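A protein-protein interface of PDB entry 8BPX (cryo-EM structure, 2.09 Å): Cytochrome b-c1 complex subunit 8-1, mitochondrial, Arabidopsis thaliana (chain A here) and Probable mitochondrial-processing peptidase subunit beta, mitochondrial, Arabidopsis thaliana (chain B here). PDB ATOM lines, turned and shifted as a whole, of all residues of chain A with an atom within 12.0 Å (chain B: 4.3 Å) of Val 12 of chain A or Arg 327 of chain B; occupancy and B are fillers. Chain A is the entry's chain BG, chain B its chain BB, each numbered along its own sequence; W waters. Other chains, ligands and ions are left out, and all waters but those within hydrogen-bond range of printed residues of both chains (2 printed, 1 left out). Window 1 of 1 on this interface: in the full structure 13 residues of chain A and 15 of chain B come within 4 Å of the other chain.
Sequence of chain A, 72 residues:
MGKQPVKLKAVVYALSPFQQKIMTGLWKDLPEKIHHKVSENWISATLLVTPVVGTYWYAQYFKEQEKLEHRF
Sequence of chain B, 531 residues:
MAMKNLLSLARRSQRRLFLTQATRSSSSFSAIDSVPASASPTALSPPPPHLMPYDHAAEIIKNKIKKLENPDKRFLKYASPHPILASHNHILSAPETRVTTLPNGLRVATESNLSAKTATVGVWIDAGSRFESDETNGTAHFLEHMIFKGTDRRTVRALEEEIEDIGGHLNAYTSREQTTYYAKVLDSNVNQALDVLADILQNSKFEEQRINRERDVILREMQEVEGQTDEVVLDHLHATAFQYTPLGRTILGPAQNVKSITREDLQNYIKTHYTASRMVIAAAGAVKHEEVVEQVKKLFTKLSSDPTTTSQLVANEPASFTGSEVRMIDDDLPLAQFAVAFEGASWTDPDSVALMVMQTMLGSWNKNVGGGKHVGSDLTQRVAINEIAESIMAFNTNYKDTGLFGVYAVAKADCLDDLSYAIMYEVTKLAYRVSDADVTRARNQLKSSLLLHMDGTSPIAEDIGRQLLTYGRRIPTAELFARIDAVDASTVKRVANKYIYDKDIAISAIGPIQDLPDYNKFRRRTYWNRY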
ATOM      1  N   LEU A   8     -23.225  -4.142 -31.794  1.00  0.00           N
ATOM      2  CA  LEU A   8     -22.971  -4.528 -30.414  1.00  0.00           C
ATOM      3  C   LEU A   8     -22.396  -3.347 -29.644  1.00  0.00           C
ATOM      4  O   LEU A   8     -21.587  -2.581 -30.177  1.00  0.00           O
ATOM      5  CB  LEU A   8     -22.009  -5.720 -30.365  1.00  0.00           C
ATOM      6  CG  LEU A   8     -21.651  -6.400 -29.038  1.00  0.00           C
ATOM      7  CD1 LEU A   8     -20.436  -5.754 -28.394  1.00  0.00           C
ATOM      8  CD2 LEU A   8     -22.841  -6.401 -28.084  1.00  0.00           C
ATOM      9  N   LYS A   9     -22.824  -3.195 -28.394  1.00  0.00           N
ATOM     10  CA  LYS A   9     -22.207  -2.252 -27.472  1.00  0.00           C
ATOM     11  C   LYS A   9     -21.804  -3.048 -26.238  1.00  0.00           C
ATOM     12  O   LYS A   9     -22.655  -3.667 -25.593  1.00  0.00           O
ATOM     13  CB  LYS A   9     -23.170  -1.118 -27.102  1.00  0.00           C
ATOM     14  CG  LYS A   9     -22.610  -0.006 -26.180  1.00  0.00           C
ATOM     15  CD  LYS A   9     -23.559   1.143 -25.856  1.00  0.00           C
ATOM     16  CE  LYS A   9     -22.929   2.158 -24.936  1.00  0.00           C
ATOM     17  NZ  LYS A   9     -23.862   3.275 -24.624  1.00  0.00           N
ATOM     18  N   ALA A  10     -20.516  -3.017 -25.906  1.00  0.00           N
ATOM     19  CA  ALA A  10     -20.024  -3.699 -24.718  1.00  0.00           C
ATOM     20  C   ALA A  10     -18.632  -3.183 -24.390  1.00  0.00           C
ATOM     21  O   ALA A  10     -17.940  -2.622 -25.243  1.00  0.00           O
ATOM     22  CB  ALA A  10     -19.997  -5.219 -24.907  1.00  0.00           C
ATOM     23  N   VAL A  11     -18.231  -3.379 -23.137  1.00  0.00           N
ATOM     24  CA  VAL A  11     -16.867  -3.137 -22.690  1.00  0.00           C
ATOM     25  C   VAL A  11     -16.308  -4.459 -22.187  1.00  0.00           C
ATOM     26  O   VAL A  11     -16.943  -5.134 -21.370  1.00  0.00           O
ATOM     27  CB  VAL A  11     -16.797  -2.054 -21.598  1.00  0.00           C
ATOM     28  CG1 VAL A  11     -15.385  -1.949 -21.054  1.00  0.00           C
ATOM     29  CG2 VAL A  11     -17.257  -0.716 -22.147  1.00  0.00           C
ATOM     30  N   VAL A  12     -15.138  -4.840 -22.690  1.00  0.00           N
ATOM     31  CA  VAL A  12     -14.507  -6.110 -22.355  1.00  0.00           C
ATOM     32  C   VAL A  12     -13.119  -5.832 -21.801  1.00  0.00           C
ATOM     33  O   VAL A  12     -12.279  -5.234 -22.484  1.00  0.00           O
ATOM     34  CB  VAL A  12     -14.430  -7.052 -23.568  1.00  0.00           C
ATOM     35  CG1 VAL A  12     -14.035  -8.447 -23.129  1.00  0.00           C
ATOM     36  CG2 VAL A  12     -15.758  -7.083 -24.304  1.00  0.00           C
ATOM     37  N   TYR A  13     -12.917  -6.271 -20.572  1.00  0.00           N
ATOM     38  CA  TYR A  13     -11.585  -6.166 -19.952  1.00  0.00           C
ATOM     39  C   TYR A  13     -11.000  -7.570 -19.929  1.00  0.00           C
ATOM     40  O   TYR A  13     -11.715  -8.496 -19.547  1.00  0.00           O
ATOM     41  CB  TYR A  13     -11.658  -5.555 -18.556  1.00  0.00           C
ATOM     42  CG  TYR A  13     -12.513  -4.334 -18.370  1.00  0.00           C
ATOM     43  CD1 TYR A  13     -13.887  -4.440 -18.246  1.00  0.00           C
ATOM     44  CD2 TYR A  13     -11.941  -3.081 -18.250  1.00  0.00           C
ATOM     45  CE1 TYR A  13     -14.674  -3.324 -18.043  1.00  0.00           C
ATOM     46  CE2 TYR A  13     -12.714  -1.952 -18.051  1.00  0.00           C
ATOM     47  CZ  TYR A  13     -14.085  -2.079 -17.939  1.00  0.00           C
ATOM     48  OH  TYR A  13     -14.866  -0.980 -17.755  1.00  0.00           O
ATOM     49  N   ALA A  14      -9.755  -7.707 -20.350  1.00  0.00           N
ATOM     50  CA  ALA A  14      -9.091  -9.016 -20.401  1.00  0.00           C
ATOM     51  C   ALA A  14      -7.677  -8.936 -19.831  1.00  0.00           C
ATOM     52  O   ALA A  14      -7.042  -7.885 -19.936  1.00  0.00           O
ATOM     53  CB  ALA A  14      -9.128  -9.575 -21.794  1.00  0.00           C
ATOM     54  N   LEU A  15      -7.244 -10.009 -19.191  1.00  0.00           N
ATOM     55  CA  LEU A  15      -5.886 -10.097 -18.642  1.00  0.00           C
ATOM     56  C   LEU A  15      -5.091 -11.067 -19.514  1.00  0.00           C
ATOM     57  O   LEU A  15      -5.677 -11.990 -20.064  1.00  0.00           O
ATOM     58  CB  LEU A  15      -6.000 -10.557 -17.184  1.00  0.00           C
ATOM     59  CG  LEU A  15      -4.717 -10.603 -16.364  1.00  0.00           C
ATOM     60  CD1 LEU A  15      -4.100  -9.222 -16.253  1.00  0.00           C
ATOM     61  CD2 LEU A  15      -4.993 -11.176 -14.980  1.00  0.00           C
ATOM     62  N   SER A  16      -3.797 -10.867 -19.586  1.00  0.00           N
ATOM     63  CA  SER A  16      -2.917 -11.674 -20.416  1.00  0.00           C
ATOM     64  C   SER A  16      -2.808 -13.092 -19.856  1.00  0.00           C
ATOM     65  O   SER A  16      -2.793 -13.278 -18.636  1.00  0.00           O
ATOM     66  CB  SER A  16      -1.530 -11.037 -20.502  1.00  0.00           C
ATOM     67  OG  SER A  16      -0.651 -11.835 -21.268  1.00  0.00           O
ATOM     68  N   PRO A  17      -2.717 -14.108 -20.719  1.00  0.00           N
ATOM     69  CA  PRO A  17      -2.615 -15.492 -20.219  1.00  0.00           C
ATOM     70  C   PRO A  17      -1.395 -15.741 -19.355  1.00  0.00           C
ATOM     71  O   PRO A  17      -1.416 -16.655 -18.524  1.00  0.00           O
ATOM     72  CB  PRO A  17      -2.567 -16.332 -21.505  1.00  0.00           C
ATOM     73  CG  PRO A  17      -3.044 -15.445 -22.593  1.00  0.00           C
ATOM     74  CD  PRO A  17      -2.756 -14.038 -22.188  1.00  0.00           C
ATOM     75  N   GLN A  20      -1.792 -15.115 -15.163  1.00  0.00           N
ATOM     76  CA  GLN A  20      -2.774 -15.830 -14.360  1.00  0.00           C
ATOM     77  C   GLN A  20      -2.378 -17.295 -14.232  1.00  0.00           C
ATOM     78  O   GLN A  20      -1.649 -17.839 -15.064  1.00  0.00           O
ATOM     79  CB  GLN A  20      -4.193 -15.712 -14.942  1.00  0.00           C
ATOM     80  CG  GLN A  20      -4.257 -15.527 -16.447  1.00  0.00           C
ATOM     81  CD  GLN A  20      -5.651 -15.175 -16.939  1.00  0.00           C
ATOM     82  OE1 GLN A  20      -6.649 -15.556 -16.333  1.00  0.00           O
ATOM     83  NE2 GLN A  20      -5.722 -14.458 -18.055  1.00  0.00           N
ATOM     84  N   GLU B 325      -5.986  -5.759 -21.828  1.00  0.00           N
ATOM     85  CA  GLU B 325      -6.654  -4.931 -22.819  1.00  0.00           C
ATOM     86  C   GLU B 325      -8.038  -4.533 -22.328  1.00  0.00           C
ATOM     87  O   GLU B 325      -8.675  -5.255 -21.557  1.00  0.00           O
ATOM     88  CB  GLU B 325      -6.766  -5.642 -24.174  1.00  0.00           C
ATOM     89  CG  GLU B 325      -7.294  -7.059 -24.110  1.00  0.00           C
ATOM     90  CD  GLU B 325      -7.822  -7.539 -25.445  1.00  0.00           C
ATOM     91  OE1 GLU B 325      -7.224  -7.183 -26.481  1.00  0.00           O
ATOM     92  OE2 GLU B 325      -8.823  -8.282 -25.465  1.00  0.00           O
ATOM     93  N   VAL B 326      -8.490  -3.372 -22.792  1.00  0.00           N
ATOM     94  CA  VAL B 326      -9.864  -2.919 -22.621  1.00  0.00           C
ATOM     95  C   VAL B 326     -10.428  -2.589 -23.998  1.00  0.00           C
ATOM     96  O   VAL B 326      -9.819  -1.830 -24.759  1.00  0.00           O
ATOM     97  CB  VAL B 326      -9.959  -1.714 -21.657  1.00  0.00           C
ATOM     98  CG1 VAL B 326      -9.037  -0.577 -22.084  1.00  0.00           C
ATOM     99  CG2 VAL B 326     -11.395  -1.225 -21.541  1.00  0.00           C
ATOM    100  N   ARG B 327     -11.571  -3.187 -24.330  1.00  0.00           N
ATOM    101  CA  ARG B 327     -12.232  -2.990 -25.616  1.00  0.00           C
ATOM    102  C   ARG B 327     -13.594  -2.353 -25.371  1.00  0.00           C
ATOM    103  O   ARG B 327     -14.481  -2.983 -24.786  1.00  0.00           O
ATOM    104  CB  ARG B 327     -12.380  -4.313 -26.373  1.00  0.00           C
ATOM    105  CG  ARG B 327     -11.132  -4.771 -27.109  1.00  0.00           C
ATOM    106  CD  ARG B 327     -11.201  -6.251 -27.456  1.00  0.00           C
ATOM    107  NE  ARG B 327      -9.880  -6.814 -27.704  1.00  0.00           N
ATOM    108  CZ  ARG B 327      -9.271  -6.829 -28.882  1.00  0.00           C
ATOM    109  NH1 ARG B 327      -9.865  -6.382 -29.974  1.00  0.00           N
ATOM    110  NH2 ARG B 327      -8.032  -7.305 -28.965  1.00  0.00           N
ATOM    111  N   MET B 328     -13.762  -1.112 -25.820  1.00  0.00           N
ATOM    112  CA  MET B 328     -15.028  -0.389 -25.689  1.00  0.00           C
ATOM    113  C   MET B 328     -15.737  -0.450 -27.040  1.00  0.00           C
ATOM    114  O   MET B 328     -15.507   0.375 -27.921  1.00  0.00           O
ATOM    115  CB  MET B 328     -14.789   1.045 -25.227  1.00  0.00           C
ATOM    116  CG  MET B 328     -14.162   1.149 -23.842  1.00  0.00           C
ATOM    117  SD  MET B 328     -13.277   2.691 -23.541  1.00  0.00           S
ATOM    118  CE  MET B 328     -11.640   2.279 -24.141  1.00  0.00           C
ATOM    119  N   ILE B 329     -16.616  -1.436 -27.190  1.00  0.00           N
ATOM    120  CA  ILE B 329     -17.246  -1.730 -28.471  1.00  0.00           C
ATOM    121  C   ILE B 329     -18.481  -0.855 -28.643  1.00  0.00           C
ATOM    122  O   ILE B 329     -19.414  -0.915 -27.835  1.00  0.00           O
ATOM    123  CB  ILE B 329     -17.610  -3.217 -28.583  1.00  0.00           C
ATOM    124  CG1 ILE B 329     -16.353  -4.081 -28.499  1.00  0.00           C
ATOM    125  CG2 ILE B 329     -18.358  -3.484 -29.875  1.00  0.00           C
ATOM    126  CD1 ILE B 329     -16.578  -5.419 -27.846  1.00  0.00           C
ATOM    127  N   ALA B 509      -8.922   0.130 -27.118  1.00  0.00           N
ATOM    128  CA  ALA B 509      -9.637   0.306 -28.373  1.00  0.00           C
ATOM    129  C   ALA B 509     -11.065   0.762 -28.111  1.00  0.00           C
ATOM    130  O   ALA B 509     -11.668   0.412 -27.094  1.00  0.00           O
ATOM    131  CB  ALA B 509      -9.652  -0.990 -29.191  1.00  0.00           C
ATOM    132  N   ILE B 513     -15.006  -2.179 -33.391  1.00  0.00           N
ATOM    133  CA  ILE B 513     -13.722  -2.853 -33.284  1.00  0.00           C
ATOM    134  C   ILE B 513     -13.872  -4.373 -33.284  1.00  0.00           C
ATOM    135  O   ILE B 513     -12.988  -5.075 -32.804  1.00  0.00           O
ATOM    136  CB  ILE B 513     -12.946  -2.373 -32.047  1.00  0.00           C
ATOM    137  CG1 ILE B 513     -13.834  -2.442 -30.799  1.00  0.00           C
ATOM    138  CG2 ILE B 513     -12.435  -0.960 -32.256  1.00  0.00           C
ATOM    139  CD1 ILE B 513     -13.094  -2.220 -29.514  1.00  0.00           C
ATOM    140  N   LEU B 516     -11.065  -5.964 -35.037  1.00  0.00           N
ATOM    141  CA  LEU B 516      -9.762  -5.862 -34.396  1.00  0.00           C
ATOM    142  C   LEU B 516      -9.379  -7.217 -33.815  1.00  0.00           C
ATOM    143  O   LEU B 516     -10.180  -7.828 -33.099  1.00  0.00           O
ATOM    144  CB  LEU B 516      -9.770  -4.790 -33.307  1.00  0.00           C
ATOM    145  CG  LEU B 516      -8.407  -4.384 -32.735  1.00  0.00           C
ATOM    146  CD1 LEU B 516      -7.603  -3.561 -33.733  1.00  0.00           C
ATOM    147  CD2 LEU B 516      -8.567  -3.621 -31.432  1.00  0.00           C
ATOM    148  N   PRO B 517      -8.184  -7.725 -34.109  1.00  0.00           N
ATOM    149  CA  PRO B 517      -7.808  -9.061 -33.635  1.00  0.00           C
ATOM    150  C   PRO B 517      -7.685  -9.106 -32.121  1.00  0.00           C
ATOM    151  O   PRO B 517      -7.427  -8.096 -31.466  1.00  0.00           O
ATOM    152  CB  PRO B 517      -6.452  -9.311 -34.309  1.00  0.00           C
ATOM    153  CG  PRO B 517      -6.365  -8.299 -35.409  1.00  0.00           C
ATOM    154  CD  PRO B 517      -7.138  -7.116 -34.942  1.00  0.00           C
ATOM    155  N   ASP B 518      -7.871 -10.303 -31.571  1.00  0.00           N
ATOM    156  CA  ASP B 518      -7.896 -10.467 -30.125  1.00  0.00           C
ATOM    157  C   ASP B 518      -6.484 -10.384 -29.547  1.00  0.00           C
ATOM    158  O   ASP B 518      -5.487 -10.252 -30.262  1.00  0.00           O
ATOM    159  CB  ASP B 518      -8.574 -11.782 -29.741  1.00  0.00           C
ATOM    160  CG  ASP B 518      -7.954 -12.992 -30.412  1.00  0.00           C
ATOM    161  OD1 ASP B 518      -6.712 -13.106 -30.459  1.00  0.00           O
ATOM    162  OD2 ASP B 518      -8.718 -13.852 -30.881  1.00  0.00           O
ATOM    163  N   TYR B 519      -6.408 -10.470 -28.216  1.00  0.00           N
ATOM    164  CA  TYR B 519      -5.135 -10.295 -27.528  1.00  0.00           C
ATOM    165  C   TYR B 519      -4.125 -11.359 -27.937  1.00  0.00           C
ATOM    166  O   TYR B 519      -2.932 -11.069 -28.066  1.00  0.00           O
ATOM    167  CB  TYR B 519      -5.343 -10.307 -26.013  1.00  0.00           C
ATOM    168  CG  TYR B 519      -4.108  -9.904 -25.244  1.00  0.00           C
ATOM    169  CD1 TYR B 519      -3.144 -10.841 -24.903  1.00  0.00           C
ATOM    170  CD2 TYR B 519      -3.900  -8.585 -24.869  1.00  0.00           C
ATOM    171  CE1 TYR B 519      -2.013 -10.479 -24.216  1.00  0.00           C
ATOM    172  CE2 TYR B 519      -2.769  -8.215 -24.178  1.00  0.00           C
ATOM    173  CZ  TYR B 519      -1.828  -9.167 -23.854  1.00  0.00           C
ATOM    174  OH  TYR B 519      -0.700  -8.805 -23.164  1.00  0.00           O
HETATM  175  O   HOH W   1      -8.042  -5.046 -18.841  1.00  0.00           O
HETATM  176  O   HOH W   2     -18.814   0.526 -25.507  1.00  0.00           O
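O of Glu 325 of chain B lies within hydrogen-bond range of N of Ala 14 of chain A, 2.9 Å away.
The backbone NH (N) of Arg 327 of chain B sits at hydrogen-bond distance from the backbone carbonyl oxygen (O) of Val 12 of chain A (2.8 Å).
O of Ala 10 of chain A is in hydrogen-bond range of N of Ile 329 of chain B (2.6 Å).
The guanidinium group (NH2) of Arg 327 of chain B lies within salt-bridge range of the side-chain carboxylate (OE1) of Glu 325 of chain B, 2.6 Å away.
O of Val 326 of chain B is in hydrogen-bond range of N of Ala 509 of chain B (3.2 Å).
The backbone carbonyl oxygen (O) of Leu 516 of chain B sits close to the guanidinium group (NH1) of Arg 327 of chain B (3.5 Å).
The guanidinium group (NH2) of Arg 327 of chain B sits at hydrogen-bond distance from the backbone carbonyl oxygen (O) of Pro 517 of chain B, at 2.7 Å.
O of Ala 509 of chain B sits at hydrogen-bond distance from N of Met 328 of chain B, at 2.9 Å.
The backbone carbonyl oxygen (O) of Ser 16 of chain A sits at hydrogen-bond distance from the side-chain amide nitrogen (NE2) of Gln 20 of chain A (3.2 Å).
Among the printed residues, merely in contact across the chains: Lys 9 of chain A with Ile 329 of chain B (3.1 Å), Val 11 of chain A with Arg 327 of chain B (3.2 Å), Val 12 of chain A with Val 326 of chain B (3.3 Å), Leu 8 of chain A with Ile 329 of chain B (3.4 Å), Tyr 13 of chain A with Glu 325 of chain B (3.4 Å), Ala 10 of chain A with Arg 327 of chain B (3.5 Å), Ser 16 of chain A with Tyr 519 of chain B (3.5 Å), Ala 10 of chain A with Met 328 of chain B (3.6 Å), Val 12 of chain A with Glu 325 of chain B (3.7 Å), Tyr 13 of chain A with Val 326 of chain B (3.8 Å), Val 11 of chain A with Met 328 of chain B (3.99 Å) and Val 12 of chain A with Ile 329 of chain B (3.998 Å).
Of the printed residues of chain B, Val 12 of chain A touches Glu 325, Val 326, Arg 327 and Ile 329.
Arg 327 of chain B touches just these residues of chain A: Ala 10 (3.5 Å), Val 11 (3.2 Å) and Val 12 (2.8 Å).
Val 326 of chain B touches two residues of chain A.
No residue of chain A comes within 4 Å of Ile 513 of chain B.
No residue of chain A comes within 4 Å of Leu 516 of chain B.
No residue of chain A comes within 4 Å of Pro 517 of chain B.
No residue of chain A comes within 4 Å of Asp 518 of chain B.
Of the printed residues of chain B, Ser 16 of chain A touches Tyr 519.
Of the printed residues of chain B, Ala 10 of chain A touches Arg 327, Met 328 and Ile 329.
Printed residues of chain B within 4 Å of Lys 9 of chain A: Ile 329 (3.1 Å).
Of the printed residues of chain A, Tyr 519 of chain B touches Ser 16.
Gln 20 of chain A touches none of the printed residues of chain B.
The nearest printed residue of chain B that does not touch Val 12 of chain A is Met 328 of chain B (5.1 Å).
The nearest residue of chain A that does not touch Arg 327 of chain B is Tyr 13 of chain A (5.0 Å).
The nearest printed residue of chain A that does not touch Ile 329 of chain B is Val 11 of chain A (4.8 Å).
Of the 11 printed residues of chain B, 6 touch a printed residue of chain A.
Hydrophobic or aromatic side chains of chain A within 4 Å of the printed part of chain B: Leu 8, Val 11, Val 12, Tyr 13 and Ala 14.
Among the printed residues, no Asp or Glu carboxylate lies within 4 Å of a Lys or Arg side-chain nitrogen of the other chain.
Water W1 bridges the backbone carbonyl oxygen (O) of Glu 325 of chain B (2.8 Å) and the backbone carbonyl oxygen (O) of Ala 14 of chain A (3.2 Å).
Water W2 bridges O of Ile 329 of chain B (2.8 Å) and O of Ala 10 of chain A (3.3 Å).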
